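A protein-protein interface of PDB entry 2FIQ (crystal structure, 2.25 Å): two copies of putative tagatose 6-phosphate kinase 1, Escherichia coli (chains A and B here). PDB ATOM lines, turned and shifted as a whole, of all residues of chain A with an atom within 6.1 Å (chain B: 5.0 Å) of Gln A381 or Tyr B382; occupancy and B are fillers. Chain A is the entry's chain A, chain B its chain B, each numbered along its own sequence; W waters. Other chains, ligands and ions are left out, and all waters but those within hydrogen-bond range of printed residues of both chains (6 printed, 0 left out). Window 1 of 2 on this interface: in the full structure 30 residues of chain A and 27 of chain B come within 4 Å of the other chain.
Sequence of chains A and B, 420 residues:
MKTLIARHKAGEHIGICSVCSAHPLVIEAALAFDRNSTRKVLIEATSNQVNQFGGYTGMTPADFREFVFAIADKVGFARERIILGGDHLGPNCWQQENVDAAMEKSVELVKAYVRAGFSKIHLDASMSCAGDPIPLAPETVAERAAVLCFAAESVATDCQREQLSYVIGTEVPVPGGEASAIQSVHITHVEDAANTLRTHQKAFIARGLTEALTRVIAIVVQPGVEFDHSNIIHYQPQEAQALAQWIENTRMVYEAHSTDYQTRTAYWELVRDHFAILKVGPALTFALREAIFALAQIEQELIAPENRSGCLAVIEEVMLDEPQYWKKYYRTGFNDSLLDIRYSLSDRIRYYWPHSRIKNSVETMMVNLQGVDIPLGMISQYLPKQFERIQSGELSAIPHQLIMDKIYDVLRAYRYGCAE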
ATOM      1  N   GLU A 290       8.640  18.762  -5.831  1.00  0.00           N
ATOM      2  CA  GLU A 290       7.781  17.999  -6.713  1.00  0.00           C
ATOM      3  C   GLU A 290       6.503  18.768  -7.074  1.00  0.00           C
ATOM      4  O   GLU A 290       6.087  18.755  -8.227  1.00  0.00           O
ATOM      5  CB  GLU A 290       7.421  16.661  -6.091  1.00  0.00           C
ATOM      6  CG  GLU A 290       8.529  15.656  -6.062  1.00  0.00           C
ATOM      7  CD  GLU A 290       8.080  14.319  -5.520  1.00  0.00           C
ATOM      8  OE1 GLU A 290       7.062  14.262  -4.799  1.00  0.00           O
ATOM      9  OE2 GLU A 290       8.750  13.315  -5.801  1.00  0.00           O
ATOM     10  N   PHE A 293       7.518  21.575  -9.547  1.00  0.00           N
ATOM     11  CA  PHE A 293       7.866  20.981 -10.837  1.00  0.00           C
ATOM     12  C   PHE A 293       6.597  20.572 -11.551  1.00  0.00           C
ATOM     13  O   PHE A 293       6.435  20.904 -12.716  1.00  0.00           O
ATOM     14  CB  PHE A 293       8.798  19.748 -10.689  1.00  0.00           C
ATOM     15  CG  PHE A 293      10.265  20.077 -10.585  1.00  0.00           C
ATOM     16  CD1 PHE A 293      10.700  21.277 -10.026  1.00  0.00           C
ATOM     17  CD2 PHE A 293      11.228  19.139 -11.020  1.00  0.00           C
ATOM     18  CE1 PHE A 293      12.088  21.574  -9.950  1.00  0.00           C
ATOM     19  CE2 PHE A 293      12.611  19.400 -10.897  1.00  0.00           C
ATOM     20  CZ  PHE A 293      13.037  20.623 -10.367  1.00  0.00           C
ATOM     21  N   GLN A 297       5.218  22.238 -15.098  1.00  0.00           N
ATOM     22  CA  GLN A 297       4.873  21.448 -16.280  1.00  0.00           C
ATOM     23  C   GLN A 297       3.457  21.810 -16.721  1.00  0.00           C
ATOM     24  O   GLN A 297       3.208  22.053 -17.900  1.00  0.00           O
ATOM     25  CB  GLN A 297       4.939  19.961 -15.974  1.00  0.00           C
ATOM     26  CG  GLN A 297       6.349  19.363 -15.889  1.00  0.00           C
ATOM     27  CD  GLN A 297       6.334  17.890 -15.450  1.00  0.00           C
ATOM     28  OE1 GLN A 297       6.344  16.992 -16.291  1.00  0.00           O
ATOM     29  NE2 GLN A 297       6.269  17.644 -14.122  1.00  0.00           N
ATOM     30  N   TYR A 343      16.335  15.324  -8.873  1.00  0.00           N
ATOM     31  CA  TYR A 343      15.629  14.188  -8.286  1.00  0.00           C
ATOM     32  C   TYR A 343      16.326  13.553  -7.129  1.00  0.00           C
ATOM     33  O   TYR A 343      15.789  12.616  -6.553  1.00  0.00           O
ATOM     34  CB  TYR A 343      15.327  13.095  -9.337  1.00  0.00           C
ATOM     35  CG  TYR A 343      14.609  13.616 -10.547  1.00  0.00           C
ATOM     36  CD1 TYR A 343      13.310  14.162 -10.442  1.00  0.00           C
ATOM     37  CD2 TYR A 343      15.220  13.577 -11.807  1.00  0.00           C
ATOM     38  CE1 TYR A 343      12.646  14.654 -11.562  1.00  0.00           C
ATOM     39  CE2 TYR A 343      14.562  14.069 -12.935  1.00  0.00           C
ATOM     40  CZ  TYR A 343      13.289  14.601 -12.807  1.00  0.00           C
ATOM     41  OH  TYR A 343      12.648  15.070 -13.931  1.00  0.00           O
ATOM     42  N   LEU A 376      -8.796  18.952 -14.475  1.00  0.00           N
ATOM     43  CA  LEU A 376      -8.683  17.762 -13.632  1.00  0.00           C
ATOM     44  C   LEU A 376      -7.702  16.708 -14.142  1.00  0.00           C
ATOM     45  O   LEU A 376      -6.985  16.080 -13.358  1.00  0.00           O
ATOM     46  CB  LEU A 376     -10.061  17.105 -13.510  1.00  0.00           C
ATOM     47  CG  LEU A 376     -11.059  17.848 -12.639  1.00  0.00           C
ATOM     48  CD1 LEU A 376     -12.404  17.120 -12.721  1.00  0.00           C
ATOM     49  CD2 LEU A 376     -10.541  17.945 -11.207  1.00  0.00           C
ATOM     50  N   GLY A 377      -7.716  16.482 -15.450  1.00  0.00           N
ATOM     51  CA  GLY A 377      -6.820  15.524 -16.058  1.00  0.00           C
ATOM     52  C   GLY A 377      -5.356  15.907 -15.911  1.00  0.00           C
ATOM     53  O   GLY A 377      -4.501  15.041 -15.823  1.00  0.00           O
ATOM     54  N   MET A 378      -5.060  17.203 -15.874  1.00  0.00           N
ATOM     55  CA  MET A 378      -3.669  17.636 -15.664  1.00  0.00           C
ATOM     56  C   MET A 378      -3.259  17.396 -14.214  1.00  0.00           C
ATOM     57  O   MET A 378      -2.133  17.038 -13.944  1.00  0.00           O
ATOM     58  CB  MET A 378      -3.465  19.096 -16.066  1.00  0.00           C
ATOM     59  CG  MET A 378      -3.678  19.313 -17.519  1.00  0.00           C
ATOM     60  SD  MET A 378      -3.262  21.129 -18.097  1.00  0.00           S
ATOM     61  CE  MET A 378      -1.335  20.922 -18.295  1.00  0.00           C
ATOM     62  N   ILE A 379      -4.196  17.540 -13.281  1.00  0.00           N
ATOM     63  CA  ILE A 379      -3.916  17.174 -11.907  1.00  0.00           C
ATOM     64  C   ILE A 379      -3.687  15.663 -11.747  1.00  0.00           C
ATOM     65  O   ILE A 379      -2.744  15.249 -11.073  1.00  0.00           O
ATOM     66  CB  ILE A 379      -4.947  17.735 -10.932  1.00  0.00           C
ATOM     67  CG1 ILE A 379      -5.063  19.261 -11.131  1.00  0.00           C
ATOM     68  CG2 ILE A 379      -4.562  17.407  -9.463  1.00  0.00           C
ATOM     69  CD1 ILE A 379      -6.332  19.869 -10.551  1.00  0.00           C
ATOM     70  N   SER A 380      -4.528  14.841 -12.365  1.00  0.00           N
ATOM     71  CA  SER A 380      -4.337  13.398 -12.343  1.00  0.00           C
ATOM     72  C   SER A 380      -2.938  12.981 -12.877  1.00  0.00           C
ATOM     73  O   SER A 380      -2.242  12.170 -12.247  1.00  0.00           O
ATOM     74  CB  SER A 380      -5.429  12.736 -13.184  1.00  0.00           C
ATOM     75  OG  SER A 380      -5.447  11.331 -12.967  1.00  0.00           O
ATOM     76  N   GLN A 381      -2.558  13.516 -14.040  1.00  0.00           N
ATOM     77  CA  GLN A 381      -1.234  13.279 -14.619  1.00  0.00           C
ATOM     78  C   GLN A 381      -0.055  13.660 -13.705  1.00  0.00           C
ATOM     79  O   GLN A 381       0.829  12.839 -13.443  1.00  0.00           O
ATOM     80  CB  GLN A 381      -1.068  14.021 -15.949  1.00  0.00           C
ATOM     81  CG  GLN A 381       0.313  13.725 -16.622  1.00  0.00           C
ATOM     82  CD  GLN A 381       0.363  12.330 -17.210  1.00  0.00           C
ATOM     83  OE1 GLN A 381      -0.437  12.007 -18.074  1.00  0.00           O
ATOM     84  NE2 GLN A 381       1.300  11.487 -16.742  1.00  0.00           N
ATOM     85  N   TYR A 382      -0.045  14.908 -13.258  1.00  0.00           N
ATOM     86  CA  TYR A 382       1.108  15.469 -12.577  1.00  0.00           C
ATOM     87  C   TYR A 382       1.046  15.409 -11.065  1.00  0.00           C
ATOM     88  O   TYR A 382       2.094  15.393 -10.391  1.00  0.00           O
ATOM     89  CB  TYR A 382       1.354  16.893 -13.073  1.00  0.00           C
ATOM     90  CG  TYR A 382       1.641  16.905 -14.559  1.00  0.00           C
ATOM     91  CD1 TYR A 382       2.838  16.362 -15.066  1.00  0.00           C
ATOM     92  CD2 TYR A 382       0.703  17.413 -15.467  1.00  0.00           C
ATOM     93  CE1 TYR A 382       3.095  16.329 -16.439  1.00  0.00           C
ATOM     94  CE2 TYR A 382       0.964  17.425 -16.831  1.00  0.00           C
ATOM     95  CZ  TYR A 382       2.154  16.874 -17.301  1.00  0.00           C
ATOM     96  OH  TYR A 382       2.402  16.885 -18.644  1.00  0.00           O
ATOM     97  N   LEU A 383      -0.170  15.378 -10.524  1.00  0.00           N
ATOM     98  CA  LEU A 383      -0.366  15.333  -9.106  1.00  0.00           C
ATOM     99  C   LEU A 383      -1.454  14.318  -8.727  1.00  0.00           C
ATOM    100  O   LEU A 383      -2.503  14.684  -8.185  1.00  0.00           O
ATOM    101  CB  LEU A 383      -0.708  16.733  -8.595  1.00  0.00           C
ATOM    102  CG  LEU A 383       0.406  17.769  -8.804  1.00  0.00           C
ATOM    103  CD1 LEU A 383      -0.219  19.144  -8.743  1.00  0.00           C
ATOM    104  CD2 LEU A 383       1.474  17.623  -7.707  1.00  0.00           C
ATOM    105  N   PRO A 384      -1.188  13.032  -9.002  1.00  0.00           N
ATOM    106  CA  PRO A 384      -2.215  11.997  -8.883  1.00  0.00           C
ATOM    107  C   PRO A 384      -2.850  11.896  -7.496  1.00  0.00           C
ATOM    108  O   PRO A 384      -4.033  11.665  -7.409  1.00  0.00           O
ATOM    109  CB  PRO A 384      -1.468  10.694  -9.222  1.00  0.00           C
ATOM    110  CG  PRO A 384      -0.122  11.092  -9.698  1.00  0.00           C
ATOM    111  CD  PRO A 384       0.122  12.506  -9.449  1.00  0.00           C
ATOM    112  N   PHE A 387      -5.153  14.623  -7.051  1.00  0.00           N
ATOM    113  CA  PHE A 387      -6.342  14.405  -7.870  1.00  0.00           C
ATOM    114  C   PHE A 387      -7.369  13.551  -7.140  1.00  0.00           C
ATOM    115  O   PHE A 387      -8.550  13.836  -7.182  1.00  0.00           O
ATOM    116  CB  PHE A 387      -6.004  13.756  -9.220  1.00  0.00           C
ATOM    117  CG  PHE A 387      -7.235  13.298  -9.996  1.00  0.00           C
ATOM    118  CD1 PHE A 387      -8.155  14.224 -10.486  1.00  0.00           C
ATOM    119  CD2 PHE A 387      -7.480  11.941 -10.216  1.00  0.00           C
ATOM    120  CE1 PHE A 387      -9.298  13.805 -11.209  1.00  0.00           C
ATOM    121  CE2 PHE A 387      -8.621  11.509 -10.959  1.00  0.00           C
ATOM    122  CZ  PHE A 387      -9.526  12.445 -11.447  1.00  0.00           C
ATOM    123  N   ARG B 289      -2.596   5.615 -20.320  1.00  0.00           N
ATOM    124  CA  ARG B 289      -2.053   6.763 -21.013  1.00  0.00           C
ATOM    125  C   ARG B 289      -1.187   7.660 -20.100  1.00  0.00           C
ATOM    126  O   ARG B 289      -0.172   8.180 -20.546  1.00  0.00           O
ATOM    127  CB  ARG B 289      -3.218   7.524 -21.647  1.00  0.00           C
ATOM    128  CG  ARG B 289      -2.879   8.724 -22.528  1.00  0.00           C
ATOM    129  CD  ARG B 289      -3.794   9.833 -22.028  1.00  0.00           C
ATOM    130  NE  ARG B 289      -3.125  10.584 -21.002  1.00  0.00           N
ATOM    131  CZ  ARG B 289      -3.656  11.167 -19.936  1.00  0.00           C
ATOM    132  NH1 ARG B 289      -4.938  11.100 -19.616  1.00  0.00           N
ATOM    133  NH2 ARG B 289      -2.831  11.829 -19.169  1.00  0.00           N
ATOM    134  N   GLU B 290      -1.586   7.825 -18.838  1.00  0.00           N
ATOM    135  CA  GLU B 290      -0.785   8.520 -17.828  1.00  0.00           C
ATOM    136  C   GLU B 290       0.558   7.837 -17.610  1.00  0.00           C
ATOM    137  O   GLU B 290       1.576   8.509 -17.522  1.00  0.00           O
ATOM    138  CB  GLU B 290      -1.531   8.610 -16.475  1.00  0.00           C
ATOM    139  CG  GLU B 290      -2.735   9.532 -16.475  1.00  0.00           C
ATOM    140  CD  GLU B 290      -3.404   9.637 -15.122  1.00  0.00           C
ATOM    141  OE1 GLU B 290      -3.361   8.669 -14.329  1.00  0.00           O
ATOM    142  OE2 GLU B 290      -3.993  10.704 -14.862  1.00  0.00           O
ATOM    143  N   PHE B 293       2.625   8.490 -20.791  1.00  0.00           N
ATOM    144  CA  PHE B 293       3.095   9.881 -20.794  1.00  0.00           C
ATOM    145  C   PHE B 293       4.227  10.124 -19.789  1.00  0.00           C
ATOM    146  O   PHE B 293       5.169  10.857 -20.086  1.00  0.00           O
ATOM    147  CB  PHE B 293       1.927  10.837 -20.507  1.00  0.00           C
ATOM    148  CG  PHE B 293       1.122  11.207 -21.720  1.00  0.00           C
ATOM    149  CD1 PHE B 293       0.994  10.332 -22.806  1.00  0.00           C
ATOM    150  CD2 PHE B 293       0.447  12.422 -21.764  1.00  0.00           C
ATOM    151  CE1 PHE B 293       0.223  10.680 -23.935  1.00  0.00           C
ATOM    152  CE2 PHE B 293      -0.331  12.782 -22.884  1.00  0.00           C
ATOM    153  CZ  PHE B 293      -0.440  11.921 -23.960  1.00  0.00           C
ATOM    154  N   ALA B 294       4.102   9.537 -18.595  1.00  0.00           N
ATOM    155  CA  ALA B 294       5.142   9.594 -17.547  1.00  0.00           C
ATOM    156  C   ALA B 294       6.426   8.964 -18.003  1.00  0.00           C
ATOM    157  O   ALA B 294       7.516   9.510 -17.770  1.00  0.00           O
ATOM    158  CB  ALA B 294       4.652   8.896 -16.277  1.00  0.00           C
ATOM    159  N   GLN B 297       8.173  11.103 -20.678  1.00  0.00           N
ATOM    160  CA  GLN B 297       8.917  12.154 -20.001  1.00  0.00           C
ATOM    161  C   GLN B 297      10.225  11.610 -19.387  1.00  0.00           C
ATOM    162  O   GLN B 297      11.297  12.173 -19.593  1.00  0.00           O
ATOM    163  CB  GLN B 297       8.059  12.852 -18.922  1.00  0.00           C
ATOM    164  CG  GLN B 297       8.828  13.998 -18.221  1.00  0.00           C
ATOM    165  CD  GLN B 297       9.256  15.105 -19.202  1.00  0.00           C
ATOM    166  OE1 GLN B 297      10.444  15.462 -19.301  1.00  0.00           O
ATOM    167  NE2 GLN B 297       8.285  15.640 -19.936  1.00  0.00           N
ATOM    168  N   ILE B 298      10.136  10.499 -18.666  1.00  0.00           N
ATOM    169  CA  ILE B 298      11.341   9.828 -18.137  1.00  0.00           C
ATOM    170  C   ILE B 298      12.348   9.481 -19.242  1.00  0.00           C
ATOM    171  O   ILE B 298      13.555   9.685 -19.087  1.00  0.00           O
ATOM    172  CB  ILE B 298      10.958   8.549 -17.353  1.00  0.00           C
ATOM    173  CG1 ILE B 298      10.348   8.939 -16.011  1.00  0.00           C
ATOM    174  CG2 ILE B 298      12.168   7.597 -17.191  1.00  0.00           C
ATOM    175  CD1 ILE B 298       9.389   7.910 -15.437  1.00  0.00           C
ATOM    176  N   GLU B 301      14.507  12.362 -20.502  1.00  0.00           N
ATOM    177  CA  GLU B 301      15.581  12.746 -19.605  1.00  0.00           C
ATOM    178  C   GLU B 301      16.676  11.712 -19.367  1.00  0.00           C
ATOM    179  O   GLU B 301      17.779  12.078 -18.979  1.00  0.00           O
ATOM    180  CB  GLU B 301      15.003  13.208 -18.264  1.00  0.00           C
ATOM    181  CG  GLU B 301      14.112  14.407 -18.404  1.00  0.00           C
ATOM    182  CD  GLU B 301      13.547  14.883 -17.064  1.00  0.00           C
ATOM    183  OE1 GLU B 301      14.228  14.793 -16.022  1.00  0.00           O
ATOM    184  OE2 GLU B 301      12.407  15.380 -17.063  1.00  0.00           O
ATOM    185  N   TYR B 343      -5.470  15.241 -21.962  1.00  0.00           N
ATOM    186  CA  TYR B 343      -5.923  15.169 -20.576  1.00  0.00           C
ATOM    187  C   TYR B 343      -7.424  14.991 -20.349  1.00  0.00           C
ATOM    188  O   TYR B 343      -7.833  14.773 -19.217  1.00  0.00           O
ATOM    189  CB  TYR B 343      -5.464  16.409 -19.811  1.00  0.00           C
ATOM    190  CG  TYR B 343      -3.987  16.674 -19.927  1.00  0.00           C
ATOM    191  CD1 TYR B 343      -3.035  15.732 -19.476  1.00  0.00           C
ATOM    192  CD2 TYR B 343      -3.529  17.853 -20.509  1.00  0.00           C
ATOM    193  CE1 TYR B 343      -1.672  15.978 -19.586  1.00  0.00           C
ATOM    194  CE2 TYR B 343      -2.150  18.106 -20.637  1.00  0.00           C
ATOM    195  CZ  TYR B 343      -1.238  17.173 -20.171  1.00  0.00           C
ATOM    196  OH  TYR B 343       0.109  17.437 -20.328  1.00  0.00           O
ATOM    197  N   MET B 378      12.569  10.082  -9.899  1.00  0.00           N
ATOM    198  CA  MET B 378      11.754  10.346 -11.099  1.00  0.00           C
ATOM    199  C   MET B 378      10.378   9.700 -11.027  1.00  0.00           C
ATOM    200  O   MET B 378       9.401  10.218 -11.559  1.00  0.00           O
ATOM    201  CB  MET B 378      12.468   9.883 -12.376  1.00  0.00           C
ATOM    202  CG  MET B 378      13.778  10.560 -12.584  1.00  0.00           C
ATOM    203  SD  MET B 378      14.452  10.284 -14.416  1.00  0.00           S
ATOM    204  CE  MET B 378      13.223  11.166 -15.379  1.00  0.00           C
ATOM    205  N   ILE B 379      10.323   8.544 -10.382  1.00  0.00           N
ATOM    206  CA  ILE B 379       9.084   7.807 -10.204  1.00  0.00           C
ATOM    207  C   ILE B 379       8.255   8.520  -9.156  1.00  0.00           C
ATOM    208  O   ILE B 379       7.062   8.655  -9.293  1.00  0.00           O
ATOM    209  CB  ILE B 379       9.382   6.339  -9.823  1.00  0.00           C
ATOM    210  CG1 ILE B 379      10.083   5.651 -11.017  1.00  0.00           C
ATOM    211  CG2 ILE B 379       8.111   5.589  -9.394  1.00  0.00           C
ATOM    212  CD1 ILE B 379      10.549   4.251 -10.719  1.00  0.00           C
ATOM    213  N   SER B 380       8.901   9.029  -8.127  1.00  0.00           N
ATOM    214  CA  SER B 380       8.191   9.841  -7.152  1.00  0.00           C
ATOM    215  C   SER B 380       7.606  11.080  -7.853  1.00  0.00           C
ATOM    216  O   SER B 380       6.478  11.435  -7.610  1.00  0.00           O
ATOM    217  CB  SER B 380       9.123  10.211  -6.007  1.00  0.00           C
ATOM    218  OG  SER B 380       8.506  11.154  -5.175  1.00  0.00           O
ATOM    219  N   GLN B 381       8.369  11.720  -8.734  1.00  0.00           N
ATOM    220  CA  GLN B 381       7.865  12.903  -9.422  1.00  0.00           C
ATOM    221  C   GLN B 381       6.691  12.566 -10.341  1.00  0.00           C
ATOM    222  O   GLN B 381       5.632  13.184 -10.264  1.00  0.00           O
ATOM    223  CB  GLN B 381       8.980  13.603 -10.234  1.00  0.00           C
ATOM    224  CG  GLN B 381       8.473  14.834 -11.068  1.00  0.00           C
ATOM    225  CD  GLN B 381       8.198  16.043 -10.192  1.00  0.00           C
ATOM    226  OE1 GLN B 381       9.064  16.480  -9.442  1.00  0.00           O
ATOM    227  NE2 GLN B 381       6.977  16.565 -10.254  1.00  0.00           N
ATOM    228  N   TYR B 382       6.868  11.579 -11.206  1.00  0.00           N
ATOM    229  CA  TYR B 382       5.896  11.352 -12.271  1.00  0.00           C
ATOM    230  C   TYR B 382       4.853  10.261 -12.023  1.00  0.00           C
ATOM    231  O   TYR B 382       3.784  10.298 -12.633  1.00  0.00           O
ATOM    232  CB  TYR B 382       6.642  11.072 -13.574  1.00  0.00           C
ATOM    233  CG  TYR B 382       7.511  12.217 -14.004  1.00  0.00           C
ATOM    234  CD1 TYR B 382       6.958  13.446 -14.376  1.00  0.00           C
ATOM    235  CD2 TYR B 382       8.897  12.078 -14.033  1.00  0.00           C
ATOM    236  CE1 TYR B 382       7.776  14.510 -14.765  1.00  0.00           C
ATOM    237  CE2 TYR B 382       9.708  13.127 -14.412  1.00  0.00           C
ATOM    238  CZ  TYR B 382       9.143  14.329 -14.776  1.00  0.00           C
ATOM    239  OH  TYR B 382       9.989  15.341 -15.151  1.00  0.00           O
ATOM    240  N   LEU B 383       5.191   9.299 -11.153  1.00  0.00           N
ATOM    241  CA  LEU B 383       4.346   8.165 -10.794  1.00  0.00           C
ATOM    242  C   LEU B 383       4.316   7.967  -9.259  1.00  0.00           C
ATOM    243  O   LEU B 383       4.714   6.921  -8.744  1.00  0.00           O
ATOM    244  CB  LEU B 383       4.861   6.898 -11.510  1.00  0.00           C
ATOM    245  CG  LEU B 383       4.767   6.938 -13.060  1.00  0.00           C
ATOM    246  CD1 LEU B 383       5.654   5.911 -13.745  1.00  0.00           C
ATOM    247  CD2 LEU B 383       3.289   6.825 -13.587  1.00  0.00           C
ATOM    248  N   PRO B 384       3.884   8.994  -8.513  1.00  0.00           N
ATOM    249  CA  PRO B 384       4.031   8.908  -7.046  1.00  0.00           C
ATOM    250  C   PRO B 384       3.385   7.714  -6.327  1.00  0.00           C
ATOM    251  O   PRO B 384       3.976   7.193  -5.379  1.00  0.00           O
ATOM    252  CB  PRO B 384       3.432  10.236  -6.542  1.00  0.00           C
ATOM    253  CG  PRO B 384       2.691  10.802  -7.650  1.00  0.00           C
ATOM    254  CD  PRO B 384       3.338  10.296  -8.930  1.00  0.00           C
HETATM  255  O   HOH W   1       4.555  15.453 -11.826  1.00  0.00           O
HETATM  256  O   HOH W   2       3.378  12.256 -14.466  1.00  0.00           O
HETATM  257  O   HOH W   3      -9.241  17.180 -17.572  1.00  0.00           O
HETATM  258  O   HOH W   4       3.867  14.399  -8.361  1.00  0.00           O
HETATM  259  O   HOH W   5       0.980  10.244 -13.018  1.00  0.00           O
HETATM  260  O   HOH W   6      -4.143  12.644 -17.045  1.00  0.00           O
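The side-chain hydroxyl (OG) of Ser B380 sits close to the side-chain carboxylate (OE1) of Glu A290 (3.4 Å). The side-chain amide nitrogen (NE2) of Gln B381 is in hydrogen-bond range of the backbone carbonyl oxygen (O) of Glu A290 (3.1 Å). OH of Tyr A343 sits at hydrogen-bond distance from OE1 of Glu B301. The side-chain hydroxyl (OH) of Tyr B382 sits at hydrogen-bond distance from the side-chain hydroxyl (OH) of Tyr A343 (2.9 Å). The side-chain hydroxyl of Ser A380 is in hydrogen-bond range of the side-chain carboxylate of Glu B290 (2.5 Å). The side-chain amide oxygen (OE1) of Gln A381 is in hydrogen-bond range of the guanidinium group (NH2) of Arg B289, 2.6 Å away. The side-chain amide nitrogen (NE2) of Gln A381 lies within hydrogen-bond range of the backbone carbonyl oxygen (O) of Glu B290, 3.1 Å away. The side-chain hydroxyl of Tyr B343 is in hydrogen-bond range of the side-chain hydroxyl of Tyr A382, at 2.9 Å.
OE2 of Glu B301 sits close to OE1 of Gln B297 (3.0 Å). OE2 of Glu B301 is in hydrogen-bond range of OH of Tyr B382 (3.1 Å).
Gln B381 touches Phe A293. Gln A297 touches Tyr B382 (OE1 to CE1, 3.2 Å). CD2 of Tyr A343 touches CG of Met B378 (3.4 Å). Tyr B343 touches Gly A377 (O to CA, 3.4 Å). Tyr B343 touches Met A378 (CD2 to CG, 3.3 Å). CB of Phe B293 touches OE1 of Gln A381, at 3.6 Å. NE2 of Gln A381 touches N of Ala B294, at 3.9 Å. Tyr B382 touches Gln A381 (O to O, 3.98 Å). Pro A384 touches Pro B384 (CG to CG, 3.5 Å).
Of the printed residues of chain B, Phe A293 touches Gln B381. Printed residues of chain B within 4 Å of Tyr A343: Glu B301 (2.6 Å), Met B378 (3.4 Å) and Tyr B382 (2.9 Å). Leu A376 touches none of the printed residues of chain B. Printed residues of chain B within 4 Å of Ser A380: Glu B290. Of the printed residues of chain B, Gln A381 touches Arg B289, Glu B290, Phe B293, Ala B294 and Tyr B382. Of the printed residues of chain A, Arg B289 touches Gln A381 (2.6 Å). Of the printed residues of chain A, Ala B294 touches Gln A381 (3.9 Å). Ile B379 touches none of the printed residues of chain A. Of the printed residues of chain A, Tyr B382 touches Gln A297, Tyr A343 and Gln A381. The nearest printed residue of chain B that does not touch Gln A381 is Tyr B343 (4.2 Å). The nearest printed residue of chain A that does not touch Tyr B382 is Pro A384 (4.9 Å).
Of the 14 printed residues of chain A, 10 touch a printed residue of chain B. Hydrophobic or aromatic side chains of chain B within 4 Å of the printed part of chain A: Phe B293, Tyr B343, Met B378, Tyr B382 and Pro B384. Among the printed residues, no Asp or Glu carboxylate lies within 4 Å of a Lys or Arg side-chain nitrogen of the other chain.
Gln A297 touches Tyr B382, but with the chains exchanged Tyr A382 does not touch Gln B297 (6.2 Å). Tyr A343 touches Met B378, and with the chains exchanged Met A378 touches Tyr B343. Gln A381 touches Tyr B382, but with the chains exchanged Tyr A382 does not touch Gln B381 (4.2 Å). Pro A384 touches its own counterpart, Pro B384. 11 positions are printed for both chains. Of the 17 pairs that touch across the chains among the printed residues, 11 have their exchanged pair printed and touching as well.
Water W6 lies within hydrogen-bond range of NH2 of Arg B289, O of Gly A377 and OE2 of Glu B290. Water W5 lies within hydrogen-bond range of the backbone carbonyl oxygen (O) of Gln A381 and the backbone carbonyl oxygen (O) of Tyr B382. Water W3 lies within hydrogen-bond range of the backbone NH of Gly A377 and the backbone carbonyl oxygen of Tyr B343. Water W2 lies within hydrogen-bond range of O of Tyr B382 (2.7 Å) and O of Gln A381 (2.8 Å). Water W1 bridges the backbone carbonyl oxygen (O) of Tyr A382 (2.8 Å) and the backbone carbonyl oxygen (O) of Gln B381 (3.0 Å). Water W4 lies within hydrogen-bond range of the backbone carbonyl oxygen of Gln B381 and the backbone carbonyl oxygen of Tyr A382.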
